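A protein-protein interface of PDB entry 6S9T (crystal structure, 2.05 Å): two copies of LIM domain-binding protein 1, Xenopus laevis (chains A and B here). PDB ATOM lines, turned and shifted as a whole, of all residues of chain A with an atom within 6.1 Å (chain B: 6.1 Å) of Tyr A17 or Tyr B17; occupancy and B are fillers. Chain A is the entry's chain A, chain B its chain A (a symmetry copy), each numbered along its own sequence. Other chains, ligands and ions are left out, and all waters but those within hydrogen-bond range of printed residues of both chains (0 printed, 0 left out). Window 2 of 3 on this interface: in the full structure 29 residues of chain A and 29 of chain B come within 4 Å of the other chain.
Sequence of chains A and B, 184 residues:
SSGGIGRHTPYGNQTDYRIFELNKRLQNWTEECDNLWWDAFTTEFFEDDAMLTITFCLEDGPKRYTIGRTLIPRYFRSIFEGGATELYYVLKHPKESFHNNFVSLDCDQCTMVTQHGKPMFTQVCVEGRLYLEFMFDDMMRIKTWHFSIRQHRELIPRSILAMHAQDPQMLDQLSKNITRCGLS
The side-chain amide nitrogen (NE2) of Gln A14 sits at hydrogen-bond distance from the side-chain carboxylate (OD2) of Asp A16 (3.4 Å).
OD2 of Asp B16 is in hydrogen-bond range of NE2 of Gln B14 (3.4 Å).
Among the printed residues, pairs that only touch across the chains: Tyr A17 with Tyr B17 (3.0 Å), Phe A20 with Asp B16 (3.4 Å), Asp A16 with Phe B20 (3.4 Å), Phe A20 with Tyr B17 (3.5 Å), Tyr A17 with Phe B20 (3.5 Å) and Phe A20 with Phe B20 (3.6 Å).
Of the printed residues of chain B, Asp A16 touches Phe B20.
Tyr A17 touches just these residues of chain B: Tyr B17 and Phe B20.
Arg A18 touches none of the printed residues of chain B.
Of the printed residues of chain B, Phe A20 touches Asp B16 (3.4 Å), Tyr B17 (3.5 Å) and Phe B20 (3.6 Å).
Of chain A, only Tyr A17 (3.0 Å) and Phe A20 (3.5 Å) come within 4 Å of Tyr B17.
Of the printed residues of chain A, Phe B20 touches Asp A16 (3.4 Å), Tyr A17 (3.5 Å) and Phe A20 (3.6 Å).
Leu B22 touches none of the printed residues of chain A.
The nearest printed residue of chain A that does not touch Asp B16 is Tyr A17 (6.3 Å).
Of the 9 printed residues of chain B, 3 touch a printed residue of chain A.
Printed residues of chain B that touch a printed residue of chain A: Asp B16, Tyr B17 and Phe B20.
Hydrophobic or aromatic side chains of chain B within 4 Å of the printed part of chain A: Tyr B17 and Phe B20.
Among the printed residues, 6 pairs touch across the chains.
Among the printed residues, no Asp or Glu carboxylate lies within 4 Å of a Lys or Arg side-chain nitrogen of the other chain.
Asp A16 touches Phe B20, and with the chains exchanged Phe A20 touches Asp B16.
Tyr A17 touches its own counterpart, Tyr B17.
Tyr A17 touches Phe B20, and with the chains exchanged Phe A20 touches Tyr B17.
Phe A20 touches its own counterpart, Phe B20.
Of the 6 pairs that touch across the chains among the printed residues, 6 have their exchanged pair printed and touching as well.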
ATOM      1  N   GLN A  14     -33.720 -28.307   5.879  1.00  0.00           N
ATOM      2  CA  GLN A  14     -33.052 -28.879   4.668  1.00  0.00           C
ATOM      3  C   GLN A  14     -31.524 -28.808   4.860  1.00  0.00           C
ATOM      4  O   GLN A  14     -31.055 -28.046   5.722  1.00  0.00           O
ATOM      5  CB  GLN A  14     -33.558 -28.187   3.396  1.00  0.00           C
ATOM      6  CG  GLN A  14     -33.462 -26.668   3.432  1.00  0.00           C
ATOM      7  CD  GLN A  14     -33.042 -26.090   2.103  1.00  0.00           C
ATOM      8  OE1 GLN A  14     -33.551 -26.463   1.049  1.00  0.00           O
ATOM      9  NE2 GLN A  14     -32.100 -25.163   2.143  1.00  0.00           N
ATOM     10  N   THR A  15     -30.778 -29.581   4.067  1.00  0.00           N
ATOM     11  CA  THR A  15     -29.386 -30.020   4.348  1.00  0.00           C
ATOM     12  C   THR A  15     -28.380 -28.899   4.095  1.00  0.00           C
ATOM     13  O   THR A  15     -27.218 -29.037   4.528  1.00  0.00           O
ATOM     14  CB  THR A  15     -28.967 -31.195   3.455  1.00  0.00           C
ATOM     15  OG1 THR A  15     -29.058 -30.765   2.095  1.00  0.00           O
ATOM     16  CG2 THR A  15     -29.799 -32.437   3.673  1.00  0.00           C
ATOM     17  N   ASP A  16     -28.801 -27.863   3.384  1.00  0.00           N
ATOM     18  CA  ASP A  16     -27.907 -26.812   2.842  1.00  0.00           C
ATOM     19  C   ASP A  16     -27.350 -25.986   4.003  1.00  0.00           C
ATOM     20  O   ASP A  16     -26.108 -25.851   4.055  1.00  0.00           O
ATOM     21  CB  ASP A  16     -28.650 -25.985   1.783  1.00  0.00           C
ATOM     22  CG  ASP A  16     -28.846 -26.772   0.507  1.00  0.00           C
ATOM     23  OD1 ASP A  16     -27.849 -27.308   0.016  1.00  0.00           O
ATOM     24  OD2 ASP A  16     -29.996 -26.886   0.050  1.00  0.00           O
ATOM     25  N   TYR A  17     -28.243 -25.493   4.875  1.00  0.00           N
ATOM     26  CA  TYR A  17     -27.956 -24.764   6.135  1.00  0.00           C
ATOM     27  C   TYR A  17     -26.918 -25.550   6.976  1.00  0.00           C
ATOM     28  O   TYR A  17     -26.132 -24.918   7.701  1.00  0.00           O
ATOM     29  CB  TYR A  17     -29.277 -24.517   6.874  1.00  0.00           C
ATOM     30  CG  TYR A  17     -29.213 -23.853   8.235  1.00  0.00           C
ATOM     31  CD1 TYR A  17     -28.805 -22.534   8.378  1.00  0.00           C
ATOM     32  CD2 TYR A  17     -29.622 -24.519   9.383  1.00  0.00           C
ATOM     33  CE1 TYR A  17     -28.771 -21.903   9.613  1.00  0.00           C
ATOM     34  CE2 TYR A  17     -29.593 -23.905  10.630  1.00  0.00           C
ATOM     35  CZ  TYR A  17     -29.176 -22.584  10.743  1.00  0.00           C
ATOM     36  OH  TYR A  17     -29.131 -21.957  11.961  1.00  0.00           O
ATOM     37  N   ARG A  18     -26.900 -26.884   6.900  1.00  0.00           N
ATOM     38  CA  ARG A  18     -25.901 -27.702   7.642  1.00  0.00           C
ATOM     39  C   ARG A  18     -24.517 -27.338   7.101  1.00  0.00           C
ATOM     40  O   ARG A  18     -23.633 -27.079   7.922  1.00  0.00           O
ATOM     41  CB  ARG A  18     -26.230 -29.196   7.571  1.00  0.00           C
ATOM     42  CG  ARG A  18     -27.619 -29.554   8.100  1.00  0.00           C
ATOM     43  CD  ARG A  18     -27.851 -29.126   9.545  1.00  0.00           C
ATOM     44  NE  ARG A  18     -26.967 -29.909  10.405  1.00  0.00           N
ATOM     45  CZ  ARG A  18     -26.295 -29.453  11.448  1.00  0.00           C
ATOM     46  NH1 ARG A  18     -26.393 -28.193  11.834  1.00  0.00           N
ATOM     47  NH2 ARG A  18     -25.525 -30.281  12.130  1.00  0.00           N
ATOM     48  N   ILE A  19     -24.352 -27.231   5.778  1.00  0.00           N
ATOM     49  CA  ILE A  19     -22.994 -26.993   5.201  1.00  0.00           C
ATOM     50  C   ILE A  19     -22.684 -25.501   5.381  1.00  0.00           C
ATOM     51  O   ILE A  19     -21.485 -25.183   5.528  1.00  0.00           O
ATOM     52  CB  ILE A  19     -22.818 -27.515   3.756  1.00  0.00           C
ATOM     53  CG1 ILE A  19     -23.061 -29.029   3.620  1.00  0.00           C
ATOM     54  CG2 ILE A  19     -21.437 -27.153   3.219  1.00  0.00           C
ATOM     55  CD1 ILE A  19     -22.076 -29.923   4.388  1.00  0.00           C
ATOM     56  N   PHE A  20     -23.710 -24.663   5.539  1.00  0.00           N
ATOM     57  CA  PHE A  20     -23.568 -23.246   5.972  1.00  0.00           C
ATOM     58  C   PHE A  20     -22.853 -23.246   7.329  1.00  0.00           C
ATOM     59  O   PHE A  20     -21.743 -22.714   7.435  1.00  0.00           O
ATOM     60  CB  PHE A  20     -24.912 -22.511   6.000  1.00  0.00           C
ATOM     61  CG  PHE A  20     -25.002 -21.370   6.988  1.00  0.00           C
ATOM     62  CD1 PHE A  20     -24.348 -20.170   6.762  1.00  0.00           C
ATOM     63  CD2 PHE A  20     -25.733 -21.499   8.159  1.00  0.00           C
ATOM     64  CE1 PHE A  20     -24.424 -19.128   7.676  1.00  0.00           C
ATOM     65  CE2 PHE A  20     -25.792 -20.468   9.088  1.00  0.00           C
ATOM     66  CZ  PHE A  20     -25.149 -19.278   8.833  1.00  0.00           C
ATOM     67  N   GLU A  21     -23.456 -23.917   8.304  1.00  0.00           N
ATOM     68  CA  GLU A  21     -22.967 -24.015   9.701  1.00  0.00           C
ATOM     69  C   GLU A  21     -21.556 -24.624   9.730  1.00  0.00           C
ATOM     70  O   GLU A  21     -20.711 -24.110  10.462  1.00  0.00           O
ATOM     71  CB  GLU A  21     -23.992 -24.798  10.518  1.00  0.00           C
ATOM     72  CG  GLU A  21     -25.151 -23.947  11.023  1.00  0.00           C
ATOM     73  CD  GLU A  21     -26.224 -24.778  11.720  1.00  0.00           C
ATOM     74  OE1 GLU A  21     -26.826 -25.683  11.048  1.00  0.00           O
ATOM     75  OE2 GLU A  21     -26.426 -24.571  12.947  1.00  0.00           O
ATOM     76  N   LEU A  22     -21.313 -25.680   8.959  1.00  0.00           N
ATOM     77  CA  LEU A  22     -19.981 -26.335   8.891  1.00  0.00           C
ATOM     78  C   LEU A  22     -18.930 -25.317   8.414  1.00  0.00           C
ATOM     79  O   LEU A  22     -17.908 -25.182   9.107  1.00  0.00           O
ATOM     80  CB  LEU A  22     -20.075 -27.544   7.961  1.00  0.00           C
ATOM     81  CG  LEU A  22     -18.814 -28.399   7.878  1.00  0.00           C
ATOM     82  CD1 LEU A  22     -19.163 -29.883   7.840  1.00  0.00           C
ATOM     83  CD2 LEU A  22     -18.000 -28.000   6.648  1.00  0.00           C
ATOM     84  N   GLN B  14     -31.570 -16.033  13.087  1.00  0.00           N
ATOM     85  CA  GLN B  14     -30.402 -15.098  13.131  1.00  0.00           C
ATOM     86  C   GLN B  14     -29.962 -14.780  11.689  1.00  0.00           C
ATOM     87  O   GLN B  14     -30.330 -15.521  10.763  1.00  0.00           O
ATOM     88  CB  GLN B  14     -29.288 -15.669  14.017  1.00  0.00           C
ATOM     89  CG  GLN B  14     -28.867 -17.086  13.651  1.00  0.00           C
ATOM     90  CD  GLN B  14     -27.375 -17.286  13.767  1.00  0.00           C
ATOM     91  OE1 GLN B  14     -26.746 -16.889  14.744  1.00  0.00           O
ATOM     92  NE2 GLN B  14     -26.792 -17.911  12.758  1.00  0.00           N
ATOM     93  N   THR B  15     -29.188 -13.706  11.516  1.00  0.00           N
ATOM     94  CA  THR B  15     -29.017 -12.957  10.243  1.00  0.00           C
ATOM     95  C   THR B  15     -28.099 -13.697   9.273  1.00  0.00           C
ATOM     96  O   THR B  15     -28.068 -13.324   8.083  1.00  0.00           O
ATOM     97  CB  THR B  15     -28.392 -11.576  10.472  1.00  0.00           C
ATOM     98  OG1 THR B  15     -27.111 -11.770  11.077  1.00  0.00           O
ATOM     99  CG2 THR B  15     -29.246 -10.668  11.325  1.00  0.00           C
ATOM    100  N   ASP B  16     -27.351 -14.669   9.777  1.00  0.00           N
ATOM    101  CA  ASP B  16     -26.240 -15.323   9.045  1.00  0.00           C
ATOM    102  C   ASP B  16     -26.820 -16.154   7.899  1.00  0.00           C
ATOM    103  O   ASP B  16     -26.350 -15.950   6.758  1.00  0.00           O
ATOM    104  CB  ASP B  16     -25.368 -16.125  10.022  1.00  0.00           C
ATOM    105  CG  ASP B  16     -24.535 -15.211  10.894  1.00  0.00           C
ATOM    106  OD1 ASP B  16     -23.865 -14.346  10.326  1.00  0.00           O
ATOM    107  OD2 ASP B  16     -24.609 -15.340  12.128  1.00  0.00           O
ATOM    108  N   TYR B  17     -27.798 -17.018   8.216  1.00  0.00           N
ATOM    109  CA  TYR B  17     -28.597 -17.848   7.281  1.00  0.00           C
ATOM    110  C   TYR B  17     -29.153 -16.966   6.133  1.00  0.00           C
ATOM    111  O   TYR B  17     -29.313 -17.475   5.011  1.00  0.00           O
ATOM    112  CB  TYR B  17     -29.691 -18.573   8.075  1.00  0.00           C
ATOM    113  CG  TYR B  17     -30.682 -19.419   7.303  1.00  0.00           C
ATOM    114  CD1 TYR B  17     -30.288 -20.580   6.651  1.00  0.00           C
ATOM    115  CD2 TYR B  17     -32.034 -19.102   7.274  1.00  0.00           C
ATOM    116  CE1 TYR B  17     -31.190 -21.383   5.967  1.00  0.00           C
ATOM    117  CE2 TYR B  17     -32.952 -19.892   6.591  1.00  0.00           C
ATOM    118  CZ  TYR B  17     -32.529 -21.046   5.944  1.00  0.00           C
ATOM    119  OH  TYR B  17     -33.412 -21.839   5.259  1.00  0.00           O
ATOM    120  N   ARG B  18     -29.444 -15.686   6.383  1.00  0.00           N
ATOM    121  CA  ARG B  18     -29.937 -14.768   5.318  1.00  0.00           C
ATOM    122  C   ARG B  18     -28.825 -14.639   4.275  1.00  0.00           C
ATOM    123  O   ARG B  18     -29.136 -14.783   3.089  1.00  0.00           O
ATOM    124  CB  ARG B  18     -30.411 -13.432   5.900  1.00  0.00           C
ATOM    125  CG  ARG B  18     -31.512 -13.567   6.953  1.00  0.00           C
ATOM    126  CD  ARG B  18     -32.756 -14.287   6.445  1.00  0.00           C
ATOM    127  NE  ARG B  18     -33.387 -13.454   5.425  1.00  0.00           N
ATOM    128  CZ  ARG B  18     -33.920 -13.883   4.293  1.00  0.00           C
ATOM    129  NH1 ARG B  18     -33.952 -15.169   3.990  1.00  0.00           N
ATOM    130  NH2 ARG B  18     -34.450 -13.007   3.460  1.00  0.00           N
ATOM    131  N   ILE B  19     -27.568 -14.463   4.694  1.00  0.00           N
ATOM    132  CA  ILE B  19     -26.469 -14.216   3.711  1.00  0.00           C
ATOM    133  C   ILE B  19     -26.099 -15.573   3.098  1.00  0.00           C
ATOM    134  O   ILE B  19     -25.678 -15.570   1.922  1.00  0.00           O
ATOM    135  CB  ILE B  19     -25.272 -13.422   4.283  1.00  0.00           C
ATOM    136  CG1 ILE B  19     -25.662 -12.033   4.821  1.00  0.00           C
ATOM    137  CG2 ILE B  19     -24.166 -13.292   3.241  1.00  0.00           C
ATOM    138  CD1 ILE B  19     -26.202 -11.051   3.771  1.00  0.00           C
ATOM    139  N   PHE B  20     -26.403 -16.674   3.787  1.00  0.00           N
ATOM    140  CA  PHE B  20     -26.341 -18.051   3.223  1.00  0.00           C
ATOM    141  C   PHE B  20     -27.261 -18.091   1.996  1.00  0.00           C
ATOM    142  O   PHE B  20     -26.779 -18.309   0.879  1.00  0.00           O
ATOM    143  CB  PHE B  20     -26.684 -19.119   4.267  1.00  0.00           C
ATOM    144  CG  PHE B  20     -27.276 -20.395   3.712  1.00  0.00           C
ATOM    145  CD1 PHE B  20     -26.495 -21.312   3.027  1.00  0.00           C
ATOM    146  CD2 PHE B  20     -28.625 -20.678   3.862  1.00  0.00           C
ATOM    147  CE1 PHE B  20     -27.043 -22.477   2.508  1.00  0.00           C
ATOM    148  CE2 PHE B  20     -29.183 -21.831   3.325  1.00  0.00           C
ATOM    149  CZ  PHE B  20     -28.383 -22.736   2.664  1.00  0.00           C
ATOM    150  N   GLU B  21     -28.537 -17.792   2.214  1.00  0.00           N
ATOM    151  CA  GLU B  21     -29.605 -17.809   1.186  1.00  0.00           C
ATOM    152  C   GLU B  21     -29.252 -16.851   0.036  1.00  0.00           C
ATOM    153  O   GLU B  21     -29.430 -17.233  -1.120  1.00  0.00           O
ATOM    154  CB  GLU B  21     -30.935 -17.491   1.864  1.00  0.00           C
ATOM    155  CG  GLU B  21     -31.594 -18.702   2.514  1.00  0.00           C
ATOM    156  CD  GLU B  21     -32.850 -18.333   3.297  1.00  0.00           C
ATOM    157  OE1 GLU B  21     -32.739 -17.524   4.280  1.00  0.00           O
ATOM    158  OE2 GLU B  21     -33.952 -18.797   2.898  1.00  0.00           O
ATOM    159  N   LEU B  22     -28.768 -15.651   0.346  1.00  0.00           N
ATOM    160  CA  LEU B  22     -28.374 -14.654  -0.684  1.00  0.00           C
ATOM    161  C   LEU B  22     -27.269 -15.245  -1.575  1.00  0.00           C
ATOM    162  O   LEU B  22     -27.447 -15.214  -2.804  1.00  0.00           O
ATOM    163  CB  LEU B  22     -27.922 -13.374   0.020  1.00  0.00           C
ATOM    164  CG  LEU B  22     -27.597 -12.206  -0.905  1.00  0.00           C
ATOM    165  CD1 LEU B  22     -28.105 -10.892  -0.322  1.00  0.00           C
ATOM    166  CD2 LEU B  22     -26.090 -12.146  -1.149  1.00  0.00           C
